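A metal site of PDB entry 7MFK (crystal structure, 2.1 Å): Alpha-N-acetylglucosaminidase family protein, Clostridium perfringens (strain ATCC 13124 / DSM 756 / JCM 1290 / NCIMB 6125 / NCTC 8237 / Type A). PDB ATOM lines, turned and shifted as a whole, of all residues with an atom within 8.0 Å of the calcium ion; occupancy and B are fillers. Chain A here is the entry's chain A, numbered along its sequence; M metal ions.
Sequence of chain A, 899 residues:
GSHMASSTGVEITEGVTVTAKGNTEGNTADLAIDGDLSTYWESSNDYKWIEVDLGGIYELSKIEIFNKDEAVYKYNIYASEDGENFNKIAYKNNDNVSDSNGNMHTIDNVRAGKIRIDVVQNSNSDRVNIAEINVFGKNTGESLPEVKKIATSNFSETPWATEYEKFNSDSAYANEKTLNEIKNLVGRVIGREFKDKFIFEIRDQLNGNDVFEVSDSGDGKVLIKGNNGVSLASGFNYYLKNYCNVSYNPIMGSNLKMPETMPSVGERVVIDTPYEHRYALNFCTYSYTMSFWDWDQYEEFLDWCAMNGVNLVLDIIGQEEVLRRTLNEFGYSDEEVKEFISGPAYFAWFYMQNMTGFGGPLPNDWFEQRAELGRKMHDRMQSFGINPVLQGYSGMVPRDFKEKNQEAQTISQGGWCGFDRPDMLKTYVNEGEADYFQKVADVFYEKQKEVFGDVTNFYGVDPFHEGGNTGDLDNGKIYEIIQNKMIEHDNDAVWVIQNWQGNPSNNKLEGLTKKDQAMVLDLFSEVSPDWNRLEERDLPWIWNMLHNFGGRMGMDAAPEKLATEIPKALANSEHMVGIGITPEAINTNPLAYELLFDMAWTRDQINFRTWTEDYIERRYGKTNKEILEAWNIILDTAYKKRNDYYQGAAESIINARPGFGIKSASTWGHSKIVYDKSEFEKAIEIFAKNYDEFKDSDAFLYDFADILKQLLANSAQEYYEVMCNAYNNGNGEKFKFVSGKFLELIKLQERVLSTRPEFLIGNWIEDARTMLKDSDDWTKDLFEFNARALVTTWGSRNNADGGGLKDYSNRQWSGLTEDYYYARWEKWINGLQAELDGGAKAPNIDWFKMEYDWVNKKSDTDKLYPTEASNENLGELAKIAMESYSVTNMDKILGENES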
ATOM      1  N   THR A  28       4.413  27.679   8.686  1.00  0.00           N
ATOM      2  CA  THR A  28       5.341  27.608   7.565  1.00  0.00           C
ATOM      3  C   THR A  28       4.791  26.692   6.466  1.00  0.00           C
ATOM      4  O   THR A  28       3.811  25.960   6.648  1.00  0.00           O
ATOM      5  CB  THR A  28       6.704  27.112   8.035  1.00  0.00           C
ATOM      6  OG1 THR A  28       6.595  25.760   8.494  1.00  0.00           O
ATOM      7  CG2 THR A  28       7.223  27.983   9.169  1.00  0.00           C
ATOM      8  N   ALA A  29       5.470  26.743   5.317  1.00  0.00           N
ATOM      9  CA  ALA A  29       5.041  25.998   4.143  1.00  0.00           C
ATOM     10  C   ALA A  29       4.950  24.502   4.424  1.00  0.00           C
ATOM     11  O   ALA A  29       3.974  23.846   4.061  1.00  0.00           O
ATOM     12  CB  ALA A  29       5.992  26.273   2.974  1.00  0.00           C
ATOM     13  N   ASP A  30       5.977  23.954   5.090  1.00  0.00           N
ATOM     14  CA  ASP A  30       6.045  22.519   5.335  1.00  0.00           C
ATOM     15  C   ASP A  30       4.852  21.999   6.122  1.00  0.00           C
ATOM     16  O   ASP A  30       4.585  20.791   6.091  1.00  0.00           O
ATOM     17  CB  ASP A  30       7.341  22.188   6.080  1.00  0.00           C
ATOM     18  CG  ASP A  30       7.517  23.033   7.314  1.00  0.00           C
ATOM     19  OD1 ASP A  30       7.185  22.553   8.424  1.00  0.00           O
ATOM     20  OD2 ASP A  30       7.972  24.191   7.191  1.00  0.00           O
ATOM     21  N   LEU A  31       4.134  22.868   6.838  1.00  0.00           N
ATOM     22  CA  LEU A  31       2.964  22.427   7.571  1.00  0.00           C
ATOM     23  C   LEU A  31       1.806  22.036   6.662  1.00  0.00           C
ATOM     24  O   LEU A  31       0.814  21.506   7.159  1.00  0.00           O
ATOM     25  CB  LEU A  31       2.510  23.517   8.542  1.00  0.00           C
ATOM     26  CG  LEU A  31       3.491  23.826   9.677  1.00  0.00           C
ATOM     27  CD1 LEU A  31       2.859  24.796  10.649  1.00  0.00           C
ATOM     28  CD2 LEU A  31       3.922  22.559  10.387  1.00  0.00           C
ATOM     29  N   ALA A  32       1.916  22.286   5.355  1.00  0.00           N
ATOM     30  CA  ALA A  32       0.888  21.834   4.426  1.00  0.00           C
ATOM     31  C   ALA A  32       1.105  20.389   3.960  1.00  0.00           C
ATOM     32  O   ALA A  32       0.207  19.828   3.325  1.00  0.00           O
ATOM     33  CB  ALA A  32       0.830  22.767   3.210  1.00  0.00           C
ATOM     34  N   ILE A  33       2.253  19.784   4.251  1.00  0.00           N
ATOM     35  CA  ILE A  33       2.546  18.450   3.741  1.00  0.00           C
ATOM     36  C   ILE A  33       3.075  17.546   4.848  1.00  0.00           C
ATOM     37  O   ILE A  33       3.739  16.540   4.567  1.00  0.00           O
ATOM     38  CB  ILE A  33       3.563  18.506   2.581  1.00  0.00           C
ATOM     39  CG1 ILE A  33       4.846  19.222   3.021  1.00  0.00           C
ATOM     40  CG2 ILE A  33       2.954  19.186   1.360  1.00  0.00           C
ATOM     41  CD1 ILE A  33       6.041  18.897   2.151  1.00  0.00           C
ATOM     42  N   ASP A  34       2.776  17.869   6.104  1.00  0.00           N
ATOM     43  CA  ASP A  34       3.213  17.062   7.225  1.00  0.00           C
ATOM     44  C   ASP A  34       2.195  15.992   7.634  1.00  0.00           C
ATOM     45  O   ASP A  34       2.338  15.400   8.701  1.00  0.00           O
ATOM     46  CB  ASP A  34       3.574  17.943   8.435  1.00  0.00           C
ATOM     47  CG  ASP A  34       2.367  18.665   9.011  1.00  0.00           C
ATOM     48  OD1 ASP A  34       1.269  18.604   8.428  1.00  0.00           O
ATOM     49  OD2 ASP A  34       2.526  19.316  10.070  1.00  0.00           O
ATOM     50  N   GLY A  35       1.182  15.739   6.803  1.00  0.00           N
ATOM     51  CA  GLY A  35       0.213  14.706   7.105  1.00  0.00           C
ATOM     52  C   GLY A  35      -0.645  14.978   8.323  1.00  0.00           C
ATOM     53  O   GLY A  35      -1.216  14.047   8.880  1.00  0.00           O
ATOM     54  N   ASP A  36      -0.759  16.236   8.739  1.00  0.00           N
ATOM     55  CA  ASP A  36      -1.445  16.620   9.959  1.00  0.00           C
ATOM     56  C   ASP A  36      -2.481  17.687   9.624  1.00  0.00           C
ATOM     57  O   ASP A  36      -2.121  18.837   9.346  1.00  0.00           O
ATOM     58  CB  ASP A  36      -0.453  17.138  11.000  1.00  0.00           C
ATOM     59  CG  ASP A  36      -1.056  17.283  12.374  1.00  0.00           C
ATOM     60  OD1 ASP A  36      -2.299  17.370  12.489  1.00  0.00           O
ATOM     61  OD2 ASP A  36      -0.292  17.301  13.367  1.00  0.00           O
ATOM     62  N   LEU A  37      -3.757  17.318   9.674  1.00  0.00           N
ATOM     63  CA  LEU A  37      -4.811  18.274   9.337  1.00  0.00           C
ATOM     64  C   LEU A  37      -4.941  19.407  10.357  1.00  0.00           C
ATOM     65  O   LEU A  37      -5.666  20.370  10.078  1.00  0.00           O
ATOM     66  CB  LEU A  37      -6.153  17.558   9.203  1.00  0.00           C
ATOM     67  CG  LEU A  37      -6.244  16.573   8.045  1.00  0.00           C
ATOM     68  CD1 LEU A  37      -7.535  15.794   8.151  1.00  0.00           C
ATOM     69  CD2 LEU A  37      -6.178  17.305   6.727  1.00  0.00           C
ATOM     70  N   SER A  38      -4.277  19.310  11.501  1.00  0.00           N
ATOM     71  CA  SER A  38      -4.343  20.354  12.518  1.00  0.00           C
ATOM     72  C   SER A  38      -3.280  21.425  12.350  1.00  0.00           C
ATOM     73  O   SER A  38      -3.364  22.466  13.005  1.00  0.00           O
ATOM     74  CB  SER A  38      -4.232  19.729  13.923  1.00  0.00           C
ATOM     75  OG  SER A  38      -2.987  19.078  14.088  1.00  0.00           O
ATOM     76  N   THR A  39      -2.280  21.201  11.494  1.00  0.00           N
ATOM     77  CA  THR A  39      -1.284  22.205  11.149  1.00  0.00           C
ATOM     78  C   THR A  39      -1.489  22.649   9.710  1.00  0.00           C
ATOM     79  O   THR A  39      -1.895  21.869   8.853  1.00  0.00           O
ATOM     80  CB  THR A  39       0.141  21.660  11.313  1.00  0.00           C
ATOM     81  OG1 THR A  39       0.386  20.639  10.341  1.00  0.00           O
ATOM     82  CG2 THR A  39       0.342  21.096  12.702  1.00  0.00           C
ATOM     83  N   TYR A  40      -1.177  23.918   9.450  1.00  0.00           N
ATOM     84  CA  TYR A  40      -1.468  24.475   8.142  1.00  0.00           C
ATOM     85  C   TYR A  40      -0.432  25.538   7.791  1.00  0.00           C
ATOM     86  O   TYR A  40       0.040  26.258   8.665  1.00  0.00           O
ATOM     87  CB  TYR A  40      -2.876  25.089   8.089  1.00  0.00           C
ATOM     88  CG  TYR A  40      -3.129  26.109   9.172  1.00  0.00           C
ATOM     89  CD1 TYR A  40      -3.690  25.738  10.387  1.00  0.00           C
ATOM     90  CD2 TYR A  40      -2.814  27.454   8.975  1.00  0.00           C
ATOM     91  CE1 TYR A  40      -3.931  26.679  11.381  1.00  0.00           C
ATOM     92  CE2 TYR A  40      -3.060  28.394   9.960  1.00  0.00           C
ATOM     93  CZ  TYR A  40      -3.607  27.998  11.158  1.00  0.00           C
ATOM     94  OH  TYR A  40      -3.845  28.933  12.140  1.00  0.00           O
ATOM     95  N   TRP A  41      -0.104  25.611   6.505  1.00  0.00           N
ATOM     96  CA  TRP A  41       0.508  26.814   5.980  1.00  0.00           C
ATOM     97  C   TRP A  41      -0.554  27.905   5.894  1.00  0.00           C
ATOM     98  O   TRP A  41      -1.719  27.627   5.603  1.00  0.00           O
ATOM     99  CB  TRP A  41       1.121  26.577   4.604  1.00  0.00           C
ATOM    100  CG  TRP A  41       1.422  27.844   3.871  1.00  0.00           C
ATOM    101  CD1 TRP A  41       2.479  28.675   4.089  1.00  0.00           C
ATOM    102  CD2 TRP A  41       0.643  28.439   2.831  1.00  0.00           C
ATOM    103  NE1 TRP A  41       2.414  29.751   3.242  1.00  0.00           N
ATOM    104  CE2 TRP A  41       1.303  29.628   2.450  1.00  0.00           C
ATOM    105  CE3 TRP A  41      -0.536  28.080   2.169  1.00  0.00           C
ATOM    106  CZ2 TRP A  41       0.816  30.462   1.446  1.00  0.00           C
ATOM    107  CZ3 TRP A  41      -1.016  28.900   1.173  1.00  0.00           C
ATOM    108  CH2 TRP A  41      -0.342  30.076   0.819  1.00  0.00           C
ATOM    109  N   PHE A  66      -7.009  19.973   1.686  1.00  0.00           N
ATOM    110  CA  PHE A  66      -7.751  20.289   2.888  1.00  0.00           C
ATOM    111  C   PHE A  66      -7.400  21.704   3.335  1.00  0.00           C
ATOM    112  O   PHE A  66      -6.250  22.132   3.218  1.00  0.00           O
ATOM    113  CB  PHE A  66      -7.420  19.310   4.024  1.00  0.00           C
ATOM    114  CG  PHE A  66      -7.770  17.880   3.739  1.00  0.00           C
ATOM    115  CD1 PHE A  66      -8.937  17.324   4.234  1.00  0.00           C
ATOM    116  CD2 PHE A  66      -6.903  17.083   3.003  1.00  0.00           C
ATOM    117  CE1 PHE A  66      -9.247  15.999   3.985  1.00  0.00           C
ATOM    118  CE2 PHE A  66      -7.213  15.758   2.754  1.00  0.00           C
ATOM    119  CZ  PHE A  66      -8.395  15.222   3.244  1.00  0.00           C
ATOM    120  N   ILE A 130      -3.565  26.308   3.632  1.00  0.00           N
ATOM    121  CA  ILE A 130      -3.670  24.924   3.190  1.00  0.00           C
ATOM    122  C   ILE A 130      -3.279  24.054   4.375  1.00  0.00           C
ATOM    123  O   ILE A 130      -2.163  24.144   4.884  1.00  0.00           O
ATOM    124  CB  ILE A 130      -2.768  24.638   1.976  1.00  0.00           C
ATOM    125  CG1 ILE A 130      -3.290  25.385   0.750  1.00  0.00           C
ATOM    126  CG2 ILE A 130      -2.673  23.144   1.713  1.00  0.00           C
ATOM    127  CD1 ILE A 130      -2.463  25.195  -0.500  1.00  0.00           C
ATOM    128  N   ALA A 131      -4.225  23.232   4.837  1.00  0.00           N
ATOM    129  CA  ALA A 131      -3.938  22.333   5.946  1.00  0.00           C
ATOM    130  C   ALA A 131      -3.143  21.119   5.464  1.00  0.00           C
ATOM    131  O   ALA A 131      -2.111  20.778   6.059  1.00  0.00           O
ATOM    132  CB  ALA A 131      -5.239  21.886   6.625  1.00  0.00           C
ATOM    133  N   GLU A 132      -3.597  20.479   4.396  1.00  0.00           N
ATOM    134  CA  GLU A 132      -2.885  19.341   3.828  1.00  0.00           C
ATOM    135  C   GLU A 132      -3.093  19.334   2.322  1.00  0.00           C
ATOM    136  O   GLU A 132      -4.169  19.683   1.832  1.00  0.00           O
ATOM    137  CB  GLU A 132      -3.350  18.002   4.413  1.00  0.00           C
ATOM    138  CG  GLU A 132      -2.682  17.623   5.723  1.00  0.00           C
ATOM    139  CD  GLU A 132      -1.166  17.628   5.634  1.00  0.00           C
ATOM    140  OE1 GLU A 132      -0.607  16.773   4.919  1.00  0.00           O
ATOM    141  OE2 GLU A 132      -0.540  18.483   6.290  1.00  0.00           O
ATOM    142  N   ILE A 133      -2.064  18.920   1.588  1.00  0.00           N
ATOM    143  CA  ILE A 133      -2.192  18.635   0.173  1.00  0.00           C
ATOM    144  C   ILE A 133      -1.568  17.269  -0.106  1.00  0.00           C
ATOM    145  O   ILE A 133      -0.385  17.053   0.186  1.00  0.00           O
ATOM    146  CB  ILE A 133      -1.569  19.719  -0.723  1.00  0.00           C
ATOM    147  CG1 ILE A 133      -1.617  19.286  -2.190  1.00  0.00           C
ATOM    148  CG2 ILE A 133      -0.153  20.071  -0.299  1.00  0.00           C
ATOM    149  CD1 ILE A 133      -1.411  20.404  -3.150  1.00  0.00           C
HETATM  150 CA    CA M   1      -0.701  20.074   7.987  1.00  0.00          CA
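The side-chain carboxylate (OD1) of Asp 36 lies within hydrogen-bond range of the side-chain hydroxyl (OG) of Ser 38, 2.4 Å away.
OE1 of Glu 132 lies within hydrogen-bond range of N of Gly 35.
N of Phe 66 sits at hydrogen-bond distance from O of Glu 132.
N of Ala 131 is in hydrogen-bond range of O of Phe 66, 2.8 Å away.
Six residues have an atom within 4 Å of the calcium ion: Leu 31, Asp 34, Asp 36, Thr 39, Ala 131 and Glu 132.
The nearest printed residue that does not touch the calcium ion is Tyr 40 (4.1 Å).
The calcium ion is bound by the backbone carbonyl oxygen (O) of Leu 31 (2.2 Å), the backbone carbonyl oxygen (O) of Asp 36 (2.3 Å), the backbone carbonyl oxygen (O) of Thr 39 (2.3 Å), the side-chain carboxylate (OE2) of Glu 132 (2.3 Å), the backbone carbonyl oxygen (O) of Ala 131 (2.5 Å), the side-chain carboxylate (OD1) of Asp 34 (2.5 Å) and the side-chain hydroxyl (OG1) of Thr 39 (2.7 Å).
The calcium ion has seven donor atoms within binding distance.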
